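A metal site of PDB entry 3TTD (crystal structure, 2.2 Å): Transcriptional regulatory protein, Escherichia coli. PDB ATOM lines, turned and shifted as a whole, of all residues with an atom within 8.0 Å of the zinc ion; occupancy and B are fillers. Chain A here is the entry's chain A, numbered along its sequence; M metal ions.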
ATOM      1  N   ARG A  33      15.603  24.421 -28.635  1.00  0.00           N
ATOM      2  CA  ARG A  33      16.693  23.616 -28.062  1.00  0.00           C
ATOM      3  C   ARG A  33      17.376  22.729 -29.112  1.00  0.00           C
ATOM      4  O   ARG A  33      18.596  22.491 -29.033  1.00  0.00           O
ATOM      5  CB  ARG A  33      16.163  22.752 -26.912  1.00  0.00           C
ATOM      6  CG  ARG A  33      17.209  22.155 -25.975  1.00  0.00           C
ATOM      7  CD  ARG A  33      16.531  21.572 -24.688  1.00  0.00           C
ATOM      8  NE  ARG A  33      16.040  20.198 -24.855  1.00  0.00           N
ATOM      9  CZ  ARG A  33      14.788  19.855 -25.162  1.00  0.00           C
ATOM     10  NH1 ARG A  33      13.842  20.773 -25.350  1.00  0.00           N
ATOM     11  NH2 ARG A  33      14.461  18.571 -25.265  1.00  0.00           N
ATOM     12  N   ARG A  34      16.589  22.238 -30.088  1.00  0.00           N
ATOM     13  CA  ARG A  34      17.074  21.369 -31.174  1.00  0.00           C
ATOM     14  C   ARG A  34      17.416  22.156 -32.431  1.00  0.00           C
ATOM     15  O   ARG A  34      17.541  21.576 -33.532  1.00  0.00           O
ATOM     16  CB  ARG A  34      16.046  20.280 -31.486  1.00  0.00           C
ATOM     17  CG  ARG A  34      15.902  19.262 -30.363  1.00  0.00           C
ATOM     18  CD  ARG A  34      15.211  17.986 -30.789  1.00  0.00           C
ATOM     19  NE  ARG A  34      14.934  17.136 -29.648  1.00  0.00           N
ATOM     20  CZ  ARG A  34      13.943  17.327 -28.789  1.00  0.00           C
ATOM     21  NH1 ARG A  34      13.791  16.467 -27.769  1.00  0.00           N
ATOM     22  NH2 ARG A  34      13.102  18.354 -28.931  1.00  0.00           N
ATOM     23  N   TYR A  37      20.167  20.903 -34.665  1.00  0.00           N
ATOM     24  CA  TYR A  37      20.644  19.650 -34.093  1.00  0.00           C
ATOM     25  C   TYR A  37      20.562  18.551 -35.143  1.00  0.00           C
ATOM     26  O   TYR A  37      19.466  18.227 -35.574  1.00  0.00           O
ATOM     27  CB  TYR A  37      19.811  19.255 -32.861  1.00  0.00           C
ATOM     28  CG  TYR A  37      20.405  18.047 -32.174  1.00  0.00           C
ATOM     29  CD1 TYR A  37      21.769  18.023 -31.871  1.00  0.00           C
ATOM     30  CD2 TYR A  37      19.621  16.939 -31.839  1.00  0.00           C
ATOM     31  CE1 TYR A  37      22.350  16.937 -31.251  1.00  0.00           C
ATOM     32  CE2 TYR A  37      20.199  15.810 -31.187  1.00  0.00           C
ATOM     33  CZ  TYR A  37      21.556  15.838 -30.912  1.00  0.00           C
ATOM     34  OH  TYR A  37      22.171  14.782 -30.317  1.00  0.00           O
ATOM     35  N   ARG A  59      14.195   2.153 -26.047  1.00  0.00           N
ATOM     36  CA  ARG A  59      15.497   2.813 -25.997  1.00  0.00           C
ATOM     37  C   ARG A  59      16.640   1.930 -25.443  1.00  0.00           C
ATOM     38  O   ARG A  59      17.713   1.870 -26.066  1.00  0.00           O
ATOM     39  CB  ARG A  59      15.388   4.181 -25.287  1.00  0.00           C
ATOM     40  CG  ARG A  59      16.606   5.068 -25.460  1.00  0.00           C
ATOM     41  CD  ARG A  59      16.458   6.360 -24.673  1.00  0.00           C
ATOM     42  NE  ARG A  59      17.593   7.276 -24.826  1.00  0.00           N
ATOM     43  CZ  ARG A  59      17.682   8.232 -25.744  1.00  0.00           C
ATOM     44  NH1 ARG A  59      16.692   8.445 -26.644  1.00  0.00           N
ATOM     45  NH2 ARG A  59      18.773   9.001 -25.781  1.00  0.00           N
ATOM     46  N   PHE A  67      23.080   7.094 -24.307  1.00  0.00           N
ATOM     47  CA  PHE A  67      22.775   8.511 -24.137  1.00  0.00           C
ATOM     48  C   PHE A  67      21.572   8.785 -23.192  1.00  0.00           C
ATOM     49  O   PHE A  67      20.460   9.004 -23.663  1.00  0.00           O
ATOM     50  CB  PHE A  67      22.487   9.134 -25.514  1.00  0.00           C
ATOM     51  CG  PHE A  67      23.652   9.059 -26.481  1.00  0.00           C
ATOM     52  CD1 PHE A  67      24.635  10.023 -26.466  1.00  0.00           C
ATOM     53  CD2 PHE A  67      23.745   8.007 -27.396  1.00  0.00           C
ATOM     54  CE1 PHE A  67      25.721   9.967 -27.359  1.00  0.00           C
ATOM     55  CE2 PHE A  67      24.830   7.928 -28.291  1.00  0.00           C
ATOM     56  CZ  PHE A  67      25.823   8.924 -28.268  1.00  0.00           C
ATOM     57  N   PRO A  68      21.794   8.827 -21.867  1.00  0.00           N
ATOM     58  CA  PRO A  68      20.616   9.140 -21.037  1.00  0.00           C
ATOM     59  C   PRO A  68      20.056  10.528 -21.344  1.00  0.00           C
ATOM     60  O   PRO A  68      20.824  11.473 -21.630  1.00  0.00           O
ATOM     61  CB  PRO A  68      21.145   9.065 -19.582  1.00  0.00           C
ATOM     62  CG  PRO A  68      22.488   8.370 -19.683  1.00  0.00           C
ATOM     63  CD  PRO A  68      23.017   8.622 -21.065  1.00  0.00           C
ATOM     64  N   LEU A  69      18.731  10.636 -21.304  1.00  0.00           N
ATOM     65  CA  LEU A  69      18.052  11.838 -21.707  1.00  0.00           C
ATOM     66  C   LEU A  69      18.203  12.897 -20.639  1.00  0.00           C
ATOM     67  O   LEU A  69      18.163  12.576 -19.467  1.00  0.00           O
ATOM     68  CB  LEU A  69      16.551  11.567 -21.951  1.00  0.00           C
ATOM     69  CG  LEU A  69      16.144  10.711 -23.148  1.00  0.00           C
ATOM     70  CD1 LEU A  69      14.696  10.407 -23.086  1.00  0.00           C
ATOM     71  CD2 LEU A  69      16.465  11.365 -24.480  1.00  0.00           C
ATOM     72  N   CYS A  70      18.381  14.156 -21.046  1.00  0.00           N
ATOM     73  CA  CYS A  70      18.308  15.294 -20.133  1.00  0.00           C
ATOM     74  C   CYS A  70      16.851  15.408 -19.665  1.00  0.00           C
ATOM     75  O   CYS A  70      15.975  14.750 -20.233  1.00  0.00           O
ATOM     76  CB  CYS A  70      18.756  16.569 -20.855  1.00  0.00           C
ATOM     77  SG  CYS A  70      17.519  17.229 -22.048  1.00  0.00           S
ATOM     78  N   PRO A  71      16.571  16.206 -18.611  1.00  0.00           N
ATOM     79  CA  PRO A  71      15.176  16.296 -18.151  1.00  0.00           C
ATOM     80  C   PRO A  71      14.181  16.871 -19.179  1.00  0.00           C
ATOM     81  O   PRO A  71      13.026  16.431 -19.203  1.00  0.00           O
ATOM     82  CB  PRO A  71      15.263  17.182 -16.890  1.00  0.00           C
ATOM     83  CG  PRO A  71      16.722  17.083 -16.456  1.00  0.00           C
ATOM     84  CD  PRO A  71      17.482  16.989 -17.745  1.00  0.00           C
ATOM     85  N   ALA A  72      14.602  17.810 -20.009  1.00  0.00           N
ATOM     86  CA  ALA A  72      13.678  18.424 -20.956  1.00  0.00           C
ATOM     87  C   ALA A  72      13.234  17.433 -22.017  1.00  0.00           C
ATOM     88  O   ALA A  72      12.035  17.367 -22.345  1.00  0.00           O
ATOM     89  CB  ALA A  72      14.295  19.643 -21.586  1.00  0.00           C
ATOM     90  N   CYS A  73      14.204  16.668 -22.527  1.00  0.00           N
ATOM     91  CA  CYS A  73      13.974  15.531 -23.440  1.00  0.00           C
ATOM     92  C   CYS A  73      13.079  14.425 -22.855  1.00  0.00           C
ATOM     93  O   CYS A  73      12.173  13.928 -23.516  1.00  0.00           O
ATOM     94  CB  CYS A  73      15.324  14.924 -23.852  1.00  0.00           C
ATOM     95  SG  CYS A  73      16.087  15.762 -25.253  1.00  0.00           S
ATOM     96  N   ASP A  74      13.353  14.061 -21.613  1.00  0.00           N
ATOM     97  CA  ASP A  74      12.629  13.007 -20.940  1.00  0.00           C
ATOM     98  C   ASP A  74      11.146  13.402 -20.677  1.00  0.00           C
ATOM     99  O   ASP A  74      10.235  12.570 -20.801  1.00  0.00           O
ATOM    100  CB  ASP A  74      13.381  12.655 -19.657  1.00  0.00           C
ATOM    101  CG  ASP A  74      12.835  11.421 -18.957  1.00  0.00           C
ATOM    102  OD1 ASP A  74      13.056  10.293 -19.430  1.00  0.00           O
ATOM    103  OD2 ASP A  74      12.203  11.612 -17.901  1.00  0.00           O
ATOM    104  N   GLU A  76       9.505  15.324 -22.715  1.00  0.00           N
ATOM    105  CA  GLU A  76       8.870  15.191 -24.040  1.00  0.00           C
ATOM    106  C   GLU A  76       8.609  13.721 -24.442  1.00  0.00           C
ATOM    107  O   GLU A  76       7.538  13.391 -24.993  1.00  0.00           O
ATOM    108  CB  GLU A  76       9.683  15.935 -25.114  1.00  0.00           C
ATOM    109  CG  GLU A  76       9.650  17.482 -24.948  1.00  0.00           C
ATOM    110  CD  GLU A  76      10.847  18.200 -25.611  1.00  0.00           C
ATOM    111  OE1 GLU A  76      11.658  17.556 -26.314  1.00  0.00           O
ATOM    112  OE2 GLU A  76      10.990  19.427 -25.401  1.00  0.00           O
ATOM    113  N   VAL A  90      15.080   9.668 -29.489  1.00  0.00           N
ATOM    114  CA  VAL A  90      15.064  11.127 -29.293  1.00  0.00           C
ATOM    115  C   VAL A  90      16.359  11.586 -28.599  1.00  0.00           C
ATOM    116  O   VAL A  90      16.916  10.836 -27.781  1.00  0.00           O
ATOM    117  CB  VAL A  90      13.805  11.606 -28.475  1.00  0.00           C
ATOM    118  CG1 VAL A  90      13.814  11.113 -27.038  1.00  0.00           C
ATOM    119  CG2 VAL A  90      13.662  13.160 -28.485  1.00  0.00           C
ATOM    120  N   ALA A  91      16.819  12.791 -28.923  1.00  0.00           N
ATOM    121  CA  ALA A  91      17.934  13.424 -28.246  1.00  0.00           C
ATOM    122  C   ALA A  91      17.922  14.932 -28.507  1.00  0.00           C
ATOM    123  O   ALA A  91      17.147  15.384 -29.348  1.00  0.00           O
ATOM    124  CB  ALA A  91      19.250  12.822 -28.707  1.00  0.00           C
ATOM    125  N   CYS A  92      18.718  15.703 -27.770  1.00  0.00           N
ATOM    126  CA  CYS A  92      19.000  17.125 -28.121  1.00  0.00           C
ATOM    127  C   CYS A  92      20.491  17.354 -27.964  1.00  0.00           C
ATOM    128  O   CYS A  92      21.201  16.424 -27.575  1.00  0.00           O
ATOM    129  CB  CYS A  92      18.208  18.104 -27.252  1.00  0.00           C
ATOM    130  SG  CYS A  92      18.890  18.279 -25.573  1.00  0.00           S
ATOM    131  N   PRO A  93      20.991  18.588 -28.289  1.00  0.00           N
ATOM    132  CA  PRO A  93      22.435  18.814 -28.151  1.00  0.00           C
ATOM    133  C   PRO A  93      22.990  18.569 -26.741  1.00  0.00           C
ATOM    134  O   PRO A  93      24.143  18.199 -26.611  1.00  0.00           O
ATOM    135  CB  PRO A  93      22.612  20.307 -28.554  1.00  0.00           C
ATOM    136  CG  PRO A  93      21.468  20.565 -29.432  1.00  0.00           C
ATOM    137  CD  PRO A  93      20.330  19.786 -28.835  1.00  0.00           C
ATOM    138  N   GLU A  94      22.169  18.768 -25.703  1.00  0.00           N
ATOM    139  CA  GLU A  94      22.634  18.603 -24.301  1.00  0.00           C
ATOM    140  C   GLU A  94      22.912  17.135 -23.995  1.00  0.00           C
ATOM    141  O   GLU A  94      23.950  16.792 -23.410  1.00  0.00           O
ATOM    142  CB  GLU A  94      21.623  19.165 -23.282  1.00  0.00           C
ATOM    143  CG  GLU A  94      21.251  20.639 -23.476  1.00  0.00           C
ATOM    144  CD  GLU A  94      22.476  21.546 -23.624  1.00  0.00           C
ATOM    145  OE1 GLU A  94      23.285  21.644 -22.657  1.00  0.00           O
ATOM    146  OE2 GLU A  94      22.618  22.149 -24.725  1.00  0.00           O
ATOM    147  N   CYS A  95      22.008  16.251 -24.413  1.00  0.00           N
ATOM    148  CA  CYS A  95      22.141  14.814 -24.080  1.00  0.00           C
ATOM    149  C   CYS A  95      22.455  13.839 -25.242  1.00  0.00           C
ATOM    150  O   CYS A  95      22.612  12.660 -25.018  1.00  0.00           O
ATOM    151  CB  CYS A  95      20.896  14.336 -23.354  1.00  0.00           C
ATOM    152  SG  CYS A  95      19.437  14.463 -24.364  1.00  0.00           S
ATOM    153  N   GLY A  96      22.553  14.332 -26.476  1.00  0.00           N
ATOM    154  CA  GLY A  96      22.609  13.389 -27.590  1.00  0.00           C
ATOM    155  C   GLY A  96      23.984  13.220 -28.209  1.00  0.00           C
ATOM    156  O   GLY A  96      24.984  13.719 -27.655  1.00  0.00           O
HETATM  157 ZN    ZN M   1      18.129  16.297 -24.325  1.00  0.00          ZN
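SG of Cys 73 sits close to NH2 of Arg 33 (3.2 Å). The side-chain sulfur (SG) of Cys 73 lies close to the guanidinium group (NH1) of Arg 34 (3.5 Å). The side-chain sulfur (SG) of Cys 92 lies close to the guanidinium group (NE) of Arg 33 (3.5 Å). SG of Cys 92 sits close to N of Glu 94 (3.3 Å). The backbone carbonyl oxygen (O) of Cys 92 is in hydrogen-bond range of the side-chain hydroxyl (OH) of Tyr 37 (3.3 Å). The backbone NH (N) of Ala 72 lies close to the side-chain sulfur (SG) of Cys 70 (3.6 Å).
SG of Cys 95 is bound to the zinc ion, 2.3 Å away. The side-chain sulfur (SG) of Cys 73 is bound to the zinc ion (2.3 Å). The zinc ion is bound by SG of Cys 92 (2.5 Å). The zinc ion is bound by SG of Cys 70 (2.5 Å). The zinc ion has four donor atoms within binding distance.
Four residues have an atom within 4 Å of the zinc ion: Cys 70, Cys 73, Cys 92 and Cys 95.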
